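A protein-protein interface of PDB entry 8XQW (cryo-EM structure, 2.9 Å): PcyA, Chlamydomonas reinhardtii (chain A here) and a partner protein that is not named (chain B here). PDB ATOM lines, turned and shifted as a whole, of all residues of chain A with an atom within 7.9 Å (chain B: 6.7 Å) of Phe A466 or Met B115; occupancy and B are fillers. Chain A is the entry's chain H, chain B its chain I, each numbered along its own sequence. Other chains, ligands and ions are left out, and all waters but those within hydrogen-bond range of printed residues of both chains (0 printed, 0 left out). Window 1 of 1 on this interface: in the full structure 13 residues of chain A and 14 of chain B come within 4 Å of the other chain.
NH1 of Arg B122 is in hydrogen-bond range of O of Asn A469, at 3.1 Å.
The side-chain amide oxygen (OD1) of Asn A469 sits close to the backbone carbonyl oxygen (O) of Tyr A465 (3.3 Å).
Tyr A463 touches Trp B112. Met B115 touches Tyr A463 (CE to CD2, 3.5 Å). Tyr A465 touches Arg B122. CE2 of Tyr A465 touches CE of Met B128, 3.8 Å away. Phe A466 touches Met B115 (CZ to O, 3.8 Å). CE1 of Phe A466 touches CB of Ala B118, 3.9 Å away. Phe A466 touches Ala B119. O of Pro A470 touches NH2 of Arg B122, at 3.6 Å. Arg B122 touches Ser A471.
Phe A466 touches just these residues of chain B: Met B115, Ala B118 and Ala B119. No residue of chain A comes within 4 Å of Ala B114. Printed residues of chain A within 4 Å of Ala B119: Phe A466. Printed residues of chain B within 4 Å of Tyr A465: Arg B122 (3.98 Å) and Met B128 (3.8 Å). Of the printed residues of chain A, Met B128 touches Tyr A465. The nearest residue of chain B that does not touch Phe A466 is Arg B122 (4.3 Å). The nearest printed residue of chain B that does not touch Ser A471 is Ala B118 (4.7 Å).
Of the 15 printed residues of chain A, 6 touch a printed residue of chain B. Printed residues of chain B that touch a printed residue of chain A: Trp B112, Met B115, Ala B118, Ala B119, Arg B122 and Met B128. Hydrophobic or aromatic side chains of chain B within 4 Å of the printed part of chain A: Trp B112, Met B115, Ala B118, Ala B119 and Met B128. Among the printed residues, 10 pairs touch across the chains. Among the printed residues, no Asp or Glu carboxylate lies within 4 Å of a Lys or Arg side-chain nitrogen of the other chain.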
ATOM      1  N   THR A 139      19.584 -14.897   7.837  1.00  0.00           N
ATOM      2  CA  THR A 139      18.867 -16.121   8.109  1.00  0.00           C
ATOM      3  C   THR A 139      17.401 -15.887   7.791  1.00  0.00           C
ATOM      4  O   THR A 139      16.922 -14.761   7.926  1.00  0.00           O
ATOM      5  CB  THR A 139      19.009 -16.553   9.571  1.00  0.00           C
ATOM      6  OG1 THR A 139      18.030 -15.887  10.365  1.00  0.00           O
ATOM      7  CG2 THR A 139      20.377 -16.211  10.095  1.00  0.00           C
ATOM      8  N   PRO A 140      16.668 -16.912   7.351  1.00  0.00           N
ATOM      9  CA  PRO A 140      15.299 -16.677   6.870  1.00  0.00           C
ATOM     10  C   PRO A 140      14.439 -15.849   7.800  1.00  0.00           C
ATOM     11  O   PRO A 140      13.659 -15.017   7.323  1.00  0.00           O
ATOM     12  CB  PRO A 140      14.743 -18.096   6.706  1.00  0.00           C
ATOM     13  CG  PRO A 140      15.766 -19.003   7.285  1.00  0.00           C
ATOM     14  CD  PRO A 140      17.059 -18.312   7.180  1.00  0.00           C
ATOM     15  N   PHE A 459      28.269 -29.705  19.271  1.00  0.00           N
ATOM     16  CA  PHE A 459      27.114 -29.859  18.401  1.00  0.00           C
ATOM     17  C   PHE A 459      26.423 -28.539  18.129  1.00  0.00           C
ATOM     18  O   PHE A 459      25.706 -28.428  17.132  1.00  0.00           O
ATOM     19  CB  PHE A 459      26.124 -30.853  18.995  1.00  0.00           C
ATOM     20  CG  PHE A 459      25.556 -30.438  20.311  1.00  0.00           C
ATOM     21  CD1 PHE A 459      24.440 -29.637  20.378  1.00  0.00           C
ATOM     22  CD2 PHE A 459      26.120 -30.873  21.484  1.00  0.00           C
ATOM     23  CE1 PHE A 459      23.920 -29.263  21.582  1.00  0.00           C
ATOM     24  CE2 PHE A 459      25.596 -30.504  22.689  1.00  0.00           C
ATOM     25  CZ  PHE A 459      24.498 -29.698  22.737  1.00  0.00           C
ATOM     26  N   GLU A 460      26.634 -27.535  18.977  1.00  0.00           N
ATOM     27  CA  GLU A 460      26.052 -26.223  18.740  1.00  0.00           C
ATOM     28  C   GLU A 460      26.456 -25.678  17.387  1.00  0.00           C
ATOM     29  O   GLU A 460      25.650 -25.041  16.701  1.00  0.00           O
ATOM     30  CB  GLU A 460      26.492 -25.260  19.822  1.00  0.00           C
ATOM     31  CG  GLU A 460      25.632 -25.255  21.037  1.00  0.00           C
ATOM     32  CD  GLU A 460      26.201 -24.349  22.101  1.00  0.00           C
ATOM     33  OE1 GLU A 460      26.986 -23.444  21.750  1.00  0.00           O
ATOM     34  OE2 GLU A 460      25.882 -24.544  23.291  1.00  0.00           O
ATOM     35  N   LYS A 461      27.700 -25.925  16.980  1.00  0.00           N
ATOM     36  CA  LYS A 461      28.162 -25.419  15.697  1.00  0.00           C
ATOM     37  C   LYS A 461      27.291 -25.906  14.559  1.00  0.00           C
ATOM     38  O   LYS A 461      27.178 -25.231  13.534  1.00  0.00           O
ATOM     39  CB  LYS A 461      29.606 -25.828  15.467  1.00  0.00           C
ATOM     40  CG  LYS A 461      30.592 -24.856  16.021  1.00  0.00           C
ATOM     41  CD  LYS A 461      31.989 -25.318  15.758  1.00  0.00           C
ATOM     42  CE  LYS A 461      32.265 -26.581  16.520  1.00  0.00           C
ATOM     43  NZ  LYS A 461      33.708 -26.915  16.524  1.00  0.00           N
ATOM     44  N   LEU A 462      26.661 -27.066  14.713  1.00  0.00           N
ATOM     45  CA  LEU A 462      25.739 -27.533  13.690  1.00  0.00           C
ATOM     46  C   LEU A 462      24.548 -26.604  13.580  1.00  0.00           C
ATOM     47  O   LEU A 462      24.241 -26.097  12.498  1.00  0.00           O
ATOM     48  CB  LEU A 462      25.280 -28.948  14.007  1.00  0.00           C
ATOM     49  CG  LEU A 462      25.927 -30.038  13.175  1.00  0.00           C
ATOM     50  CD1 LEU A 462      25.595 -31.376  13.752  1.00  0.00           C
ATOM     51  CD2 LEU A 462      25.428 -29.946  11.767  1.00  0.00           C
ATOM     52  N   TYR A 463      23.893 -26.331  14.704  1.00  0.00           N
ATOM     53  CA  TYR A 463      22.684 -25.521  14.682  1.00  0.00           C
ATOM     54  C   TYR A 463      22.937 -24.181  14.018  1.00  0.00           C
ATOM     55  O   TYR A 463      22.258 -23.822  13.053  1.00  0.00           O
ATOM     56  CB  TYR A 463      22.166 -25.338  16.095  1.00  0.00           C
ATOM     57  CG  TYR A 463      21.425 -26.538  16.591  1.00  0.00           C
ATOM     58  CD1 TYR A 463      22.088 -27.587  17.180  1.00  0.00           C
ATOM     59  CD2 TYR A 463      20.061 -26.622  16.465  1.00  0.00           C
ATOM     60  CE1 TYR A 463      21.417 -28.673  17.637  1.00  0.00           C
ATOM     61  CE2 TYR A 463      19.381 -27.710  16.906  1.00  0.00           C
ATOM     62  CZ  TYR A 463      20.061 -28.733  17.493  1.00  0.00           C
ATOM     63  OH  TYR A 463      19.369 -29.824  17.944  1.00  0.00           O
ATOM     64  N   THR A 464      23.946 -23.451  14.489  1.00  0.00           N
ATOM     65  CA  THR A 464      24.276 -22.179  13.864  1.00  0.00           C
ATOM     66  C   THR A 464      24.485 -22.343  12.368  1.00  0.00           C
ATOM     67  O   THR A 464      23.924 -21.581  11.575  1.00  0.00           O
ATOM     68  CB  THR A 464      25.511 -21.572  14.510  1.00  0.00           C
ATOM     69  OG1 THR A 464      26.664 -22.307  14.105  1.00  0.00           O
ATOM     70  CG2 THR A 464      25.395 -21.630  16.002  1.00  0.00           C
ATOM     71  N   TYR A 465      25.244 -23.356  11.959  1.00  0.00           N
ATOM     72  CA  TYR A 465      25.432 -23.584  10.533  1.00  0.00           C
ATOM     73  C   TYR A 465      24.094 -23.676   9.819  1.00  0.00           C
ATOM     74  O   TYR A 465      23.816 -22.915   8.889  1.00  0.00           O
ATOM     75  CB  TYR A 465      26.242 -24.852  10.310  1.00  0.00           C
ATOM     76  CG  TYR A 465      26.458 -25.181   8.864  1.00  0.00           C
ATOM     77  CD1 TYR A 465      27.412 -24.524   8.125  1.00  0.00           C
ATOM     78  CD2 TYR A 465      25.716 -26.157   8.240  1.00  0.00           C
ATOM     79  CE1 TYR A 465      27.611 -24.822   6.808  1.00  0.00           C
ATOM     80  CE2 TYR A 465      25.910 -26.458   6.926  1.00  0.00           C
ATOM     81  CZ  TYR A 465      26.855 -25.788   6.216  1.00  0.00           C
ATOM     82  OH  TYR A 465      27.053 -26.088   4.897  1.00  0.00           O
ATOM     83  N   PHE A 466      23.222 -24.543  10.295  1.00  0.00           N
ATOM     84  CA  PHE A 466      21.996 -24.764   9.557  1.00  0.00           C
ATOM     85  C   PHE A 466      20.997 -23.643   9.713  1.00  0.00           C
ATOM     86  O   PHE A 466      19.885 -23.766   9.204  1.00  0.00           O
ATOM     87  CB  PHE A 466      21.365 -26.085   9.970  1.00  0.00           C
ATOM     88  CG  PHE A 466      21.891 -27.237   9.207  1.00  0.00           C
ATOM     89  CD1 PHE A 466      21.460 -27.483   7.935  1.00  0.00           C
ATOM     90  CD2 PHE A 466      22.845 -28.050   9.747  1.00  0.00           C
ATOM     91  CE1 PHE A 466      21.961 -28.518   7.237  1.00  0.00           C
ATOM     92  CE2 PHE A 466      23.344 -29.078   9.044  1.00  0.00           C
ATOM     93  CZ  PHE A 466      22.901 -29.313   7.791  1.00  0.00           C
ATOM     94  N   ASP A 467      21.340 -22.554  10.391  1.00  0.00           N
ATOM     95  CA  ASP A 467      20.399 -21.452  10.337  1.00  0.00           C
ATOM     96  C   ASP A 467      20.799 -20.416   9.308  1.00  0.00           C
ATOM     97  O   ASP A 467      20.012 -19.513   9.028  1.00  0.00           O
ATOM     98  CB  ASP A 467      20.211 -20.830  11.725  1.00  0.00           C
ATOM     99  CG  ASP A 467      21.369 -19.961  12.167  1.00  0.00           C
ATOM    100  OD1 ASP A 467      22.264 -19.629  11.367  1.00  0.00           O
ATOM    101  OD2 ASP A 467      21.383 -19.592  13.358  1.00  0.00           O
ATOM    102  N   GLU A 468      21.994 -20.524   8.733  1.00  0.00           N
ATOM    103  CA  GLU A 468      22.375 -19.627   7.661  1.00  0.00           C
ATOM    104  C   GLU A 468      22.502 -20.314   6.313  1.00  0.00           C
ATOM    105  O   GLU A 468      22.532 -19.622   5.293  1.00  0.00           O
ATOM    106  CB  GLU A 468      23.689 -18.912   7.996  1.00  0.00           C
ATOM    107  CG  GLU A 468      24.825 -19.830   8.299  1.00  0.00           C
ATOM    108  CD  GLU A 468      25.906 -19.157   9.112  1.00  0.00           C
ATOM    109  OE1 GLU A 468      25.627 -18.090   9.695  1.00  0.00           O
ATOM    110  OE2 GLU A 468      27.035 -19.688   9.168  1.00  0.00           O
ATOM    111  N   ASN A 469      22.570 -21.640   6.273  1.00  0.00           N
ATOM    112  CA  ASN A 469      22.426 -22.411   5.043  1.00  0.00           C
ATOM    113  C   ASN A 469      21.285 -23.402   5.207  1.00  0.00           C
ATOM    114  O   ASN A 469      21.502 -24.615   5.190  1.00  0.00           O
ATOM    115  CB  ASN A 469      23.714 -23.146   4.700  1.00  0.00           C
ATOM    116  CG  ASN A 469      24.927 -22.306   4.919  1.00  0.00           C
ATOM    117  OD1 ASN A 469      25.225 -21.913   6.035  1.00  0.00           O
ATOM    118  ND2 ASN A 469      25.646 -22.027   3.849  1.00  0.00           N
ATOM    119  N   PRO A 470      20.060 -22.928   5.364  1.00  0.00           N
ATOM    120  CA  PRO A 470      18.959 -23.831   5.680  1.00  0.00           C
ATOM    121  C   PRO A 470      18.507 -24.601   4.452  1.00  0.00           C
ATOM    122  O   PRO A 470      18.996 -24.411   3.344  1.00  0.00           O
ATOM    123  CB  PRO A 470      17.871 -22.885   6.168  1.00  0.00           C
ATOM    124  CG  PRO A 470      18.111 -21.672   5.416  1.00  0.00           C
ATOM    125  CD  PRO A 470      19.591 -21.544   5.234  1.00  0.00           C
ATOM    126  N   SER A 471      17.543 -25.480   4.678  1.00  0.00           N
ATOM    127  CA  SER A 471      16.951 -26.288   3.626  1.00  0.00           C
ATOM    128  C   SER A 471      15.444 -26.249   3.775  1.00  0.00           C
ATOM    129  O   SER A 471      14.927 -26.353   4.886  1.00  0.00           O
ATOM    130  CB  SER A 471      17.455 -27.720   3.693  1.00  0.00           C
ATOM    131  OG  SER A 471      16.866 -28.499   2.682  1.00  0.00           O
ATOM    132  N   ARG B 110      12.102 -33.881  15.144  1.00  0.00           N
ATOM    133  CA  ARG B 110      11.977 -33.771  13.698  1.00  0.00           C
ATOM    134  C   ARG B 110      13.060 -32.877  13.118  1.00  0.00           C
ATOM    135  O   ARG B 110      13.632 -33.181  12.065  1.00  0.00           O
ATOM    136  CB  ARG B 110      10.596 -33.243  13.338  1.00  0.00           C
ATOM    137  CG  ARG B 110      10.377 -33.052  11.874  1.00  0.00           C
ATOM    138  CD  ARG B 110       9.231 -32.112  11.612  1.00  0.00           C
ATOM    139  NE  ARG B 110       9.596 -30.731  11.879  1.00  0.00           N
ATOM    140  CZ  ARG B 110      10.373 -30.003  11.091  1.00  0.00           C
ATOM    141  NH1 ARG B 110      10.865 -30.525   9.986  1.00  0.00           N
ATOM    142  NH2 ARG B 110      10.656 -28.756  11.410  1.00  0.00           N
ATOM    143  N   VAL B 111      13.389 -31.786  13.805  1.00  0.00           N
ATOM    144  CA  VAL B 111      14.412 -30.894  13.273  1.00  0.00           C
ATOM    145  C   VAL B 111      15.787 -31.544  13.316  1.00  0.00           C
ATOM    146  O   VAL B 111      16.580 -31.391  12.384  1.00  0.00           O
ATOM    147  CB  VAL B 111      14.399 -29.559  14.021  1.00  0.00           C
ATOM    148  CG1 VAL B 111      15.550 -28.735  13.593  1.00  0.00           C
ATOM    149  CG2 VAL B 111      13.142 -28.840  13.708  1.00  0.00           C
ATOM    150  N   TRP B 112      16.106 -32.267  14.388  1.00  0.00           N
ATOM    151  CA  TRP B 112      17.399 -32.945  14.422  1.00  0.00           C
ATOM    152  C   TRP B 112      17.532 -33.932  13.276  1.00  0.00           C
ATOM    153  O   TRP B 112      18.592 -34.036  12.648  1.00  0.00           O
ATOM    154  CB  TRP B 112      17.591 -33.661  15.742  1.00  0.00           C
ATOM    155  CG  TRP B 112      18.858 -34.419  15.837  1.00  0.00           C
ATOM    156  CD1 TRP B 112      18.991 -35.754  15.926  1.00  0.00           C
ATOM    157  CD2 TRP B 112      20.176 -33.885  15.877  1.00  0.00           C
ATOM    158  NE1 TRP B 112      20.306 -36.096  16.018  1.00  0.00           N
ATOM    159  CE2 TRP B 112      21.055 -34.957  15.996  1.00  0.00           C
ATOM    160  CE3 TRP B 112      20.698 -32.596  15.832  1.00  0.00           C
ATOM    161  CZ2 TRP B 112      22.419 -34.789  16.049  1.00  0.00           C
ATOM    162  CZ3 TRP B 112      22.048 -32.436  15.890  1.00  0.00           C
ATOM    163  CH2 TRP B 112      22.894 -33.518  16.000  1.00  0.00           C
ATOM    164  N   ASP B 113      16.465 -34.666  12.982  1.00  0.00           N
ATOM    165  CA  ASP B 113      16.546 -35.642  11.899  1.00  0.00           C
ATOM    166  C   ASP B 113      16.734 -34.969  10.550  1.00  0.00           C
ATOM    167  O   ASP B 113      17.511 -35.447   9.712  1.00  0.00           O
ATOM    168  CB  ASP B 113      15.303 -36.503  11.886  1.00  0.00           C
ATOM    169  CG  ASP B 113      15.304 -37.513  12.987  1.00  0.00           C
ATOM    170  OD1 ASP B 113      16.383 -37.759  13.557  1.00  0.00           O
ATOM    171  OD2 ASP B 113      14.227 -38.068  13.282  1.00  0.00           O
ATOM    172  N   ALA B 114      16.026 -33.869  10.308  1.00  0.00           N
ATOM    173  CA  ALA B 114      16.222 -33.165   9.047  1.00  0.00           C
ATOM    174  C   ALA B 114      17.649 -32.664   8.916  1.00  0.00           C
ATOM    175  O   ALA B 114      18.234 -32.718   7.829  1.00  0.00           O
ATOM    176  CB  ALA B 114      15.239 -32.014   8.927  1.00  0.00           C
ATOM    177  N   MET B 115      18.232 -32.177  10.009  1.00  0.00           N
ATOM    178  CA  MET B 115      19.623 -31.744   9.958  1.00  0.00           C
ATOM    179  C   MET B 115      20.542 -32.887   9.598  1.00  0.00           C
ATOM    180  O   MET B 115      21.458 -32.720   8.797  1.00  0.00           O
ATOM    181  CB  MET B 115      20.059 -31.177  11.293  1.00  0.00           C
ATOM    182  CG  MET B 115      19.434 -29.886  11.645  1.00  0.00           C
ATOM    183  SD  MET B 115      20.293 -29.183  13.022  1.00  0.00           S
ATOM    184  CE  MET B 115      19.294 -27.738  13.211  1.00  0.00           C
ATOM    185  N   ARG B 116      20.347 -34.045  10.219  1.00  0.00           N
ATOM    186  CA  ARG B 116      21.214 -35.181   9.930  1.00  0.00           C
ATOM    187  C   ARG B 116      21.166 -35.549   8.459  1.00  0.00           C
ATOM    188  O   ARG B 116      22.205 -35.768   7.830  1.00  0.00           O
ATOM    189  CB  ARG B 116      20.818 -36.368  10.784  1.00  0.00           C
ATOM    190  CG  ARG B 116      21.668 -36.524  11.978  1.00  0.00           C
ATOM    191  CD  ARG B 116      20.975 -37.342  12.982  1.00  0.00           C
ATOM    192  NE  ARG B 116      21.201 -38.750  12.770  1.00  0.00           N
ATOM    193  CZ  ARG B 116      20.240 -39.650  12.826  1.00  0.00           C
ATOM    194  NH1 ARG B 116      19.006 -39.265  13.077  1.00  0.00           N
ATOM    195  NH2 ARG B 116      20.504 -40.925  12.628  1.00  0.00           N
ATOM    196  N   VAL B 117      19.971 -35.602   7.884  1.00  0.00           N
ATOM    197  CA  VAL B 117      19.861 -35.984   6.479  1.00  0.00           C
ATOM    198  C   VAL B 117      20.539 -34.954   5.582  1.00  0.00           C
ATOM    199  O   VAL B 117      21.337 -35.299   4.700  1.00  0.00           O
ATOM    200  CB  VAL B 117      18.390 -36.183   6.094  1.00  0.00           C
ATOM    201  CG1 VAL B 117      18.245 -36.167   4.616  1.00  0.00           C
ATOM    202  CG2 VAL B 117      17.901 -37.477   6.641  1.00  0.00           C
ATOM    203  N   ALA B 118      20.236 -33.673   5.789  1.00  0.00           N
ATOM    204  CA  ALA B 118      20.807 -32.641   4.927  1.00  0.00           C
ATOM    205  C   ALA B 118      22.315 -32.555   5.076  1.00  0.00           C
ATOM    206  O   ALA B 118      23.024 -32.268   4.109  1.00  0.00           O
ATOM    207  CB  ALA B 118      20.171 -31.297   5.232  1.00  0.00           C
ATOM    208  N   ALA B 119      22.834 -32.828   6.266  1.00  0.00           N
ATOM    209  CA  ALA B 119      24.275 -32.794   6.451  1.00  0.00           C
ATOM    210  C   ALA B 119      24.938 -33.983   5.789  1.00  0.00           C
ATOM    211  O   ALA B 119      26.024 -33.852   5.226  1.00  0.00           O
ATOM    212  CB  ALA B 119      24.613 -32.757   7.934  1.00  0.00           C
ATOM    213  N   ALA B 120      24.307 -35.154   5.844  1.00  0.00           N
ATOM    214  CA  ALA B 120      24.839 -36.297   5.116  1.00  0.00           C
ATOM    215  C   ALA B 120      24.958 -35.983   3.641  1.00  0.00           C
ATOM    216  O   ALA B 120      25.978 -36.279   3.014  1.00  0.00           O
ATOM    217  CB  ALA B 120      23.947 -37.513   5.319  1.00  0.00           C
ATOM    218  N   ARG B 122      25.095 -32.897   2.084  1.00  0.00           N
ATOM    219  CA  ARG B 122      26.105 -31.877   1.829  1.00  0.00           C
ATOM    220  C   ARG B 122      27.509 -32.408   2.040  1.00  0.00           C
ATOM    221  O   ARG B 122      28.465 -31.887   1.467  1.00  0.00           O
ATOM    222  CB  ARG B 122      25.874 -30.678   2.732  1.00  0.00           C
ATOM    223  CG  ARG B 122      25.006 -29.646   2.124  1.00  0.00           C
ATOM    224  CD  ARG B 122      24.572 -28.664   3.146  1.00  0.00           C
ATOM    225  NE  ARG B 122      23.135 -28.499   3.075  1.00  0.00           N
ATOM    226  CZ  ARG B 122      22.519 -27.334   3.105  1.00  0.00           C
ATOM    227  NH1 ARG B 122      23.220 -26.226   3.217  1.00  0.00           N
ATOM    228  NH2 ARG B 122      21.204 -27.284   3.032  1.00  0.00           N
ATOM    229  N   MET B 128      31.336 -29.038   3.039  1.00  0.00           N
ATOM    230  CA  MET B 128      31.165 -29.064   4.486  1.00  0.00           C
ATOM    231  C   MET B 128      32.372 -28.408   5.154  1.00  0.00           C
ATOM    232  O   MET B 128      33.503 -28.574   4.690  1.00  0.00           O
ATOM    233  CB  MET B 128      30.969 -30.497   4.970  1.00  0.00           C
ATOM    234  CG  MET B 128      29.864 -30.664   5.991  1.00  0.00           C
ATOM    235  SD  MET B 128      28.315 -29.899   5.527  1.00  0.00           S
ATOM    236  CE  MET B 128      27.458 -29.922   7.083  1.00  0.00           C
ATOM    237  N   PHE B 132      33.607 -30.283  10.759  1.00  0.00           N
ATOM    238  CA  PHE B 132      32.518 -31.238  10.839  1.00  0.00           C
ATOM    239  C   PHE B 132      33.075 -32.632  11.064  1.00  0.00           C
ATOM    240  O   PHE B 132      33.937 -33.092  10.312  1.00  0.00           O
ATOM    241  CB  PHE B 132      31.700 -31.177   9.557  1.00  0.00           C
ATOM    242  CG  PHE B 132      30.593 -32.164   9.503  1.00  0.00           C
ATOM    243  CD1 PHE B 132      29.459 -31.990  10.255  1.00  0.00           C
ATOM    244  CD2 PHE B 132      30.683 -33.267   8.696  1.00  0.00           C
ATOM    245  CE1 PHE B 132      28.447 -32.898  10.206  1.00  0.00           C
ATOM    246  CE2 PHE B 132      29.669 -34.173   8.646  1.00  0.00           C
ATOM    247  CZ  PHE B 132      28.552 -33.989   9.401  1.00  0.00           C
ATOM    248  N   LEU B 137      26.657 -37.866  12.956  1.00  0.00           N
ATOM    249  CA  LEU B 137      25.490 -38.388  12.266  1.00  0.00           C
ATOM    250  C   LEU B 137      24.996 -39.686  12.860  1.00  0.00           C
ATOM    251  O   LEU B 137      23.977 -40.206  12.405  1.00  0.00           O
ATOM    252  CB  LEU B 137      25.802 -38.592  10.790  1.00  0.00           C
ATOM    253  CG  LEU B 137      26.293 -37.368  10.036  1.00  0.00           C
ATOM    254  CD1 LEU B 137      26.741 -37.759   8.661  1.00  0.00           C
ATOM    255  CD2 LEU B 137      25.209 -36.344   9.943  1.00  0.00           C
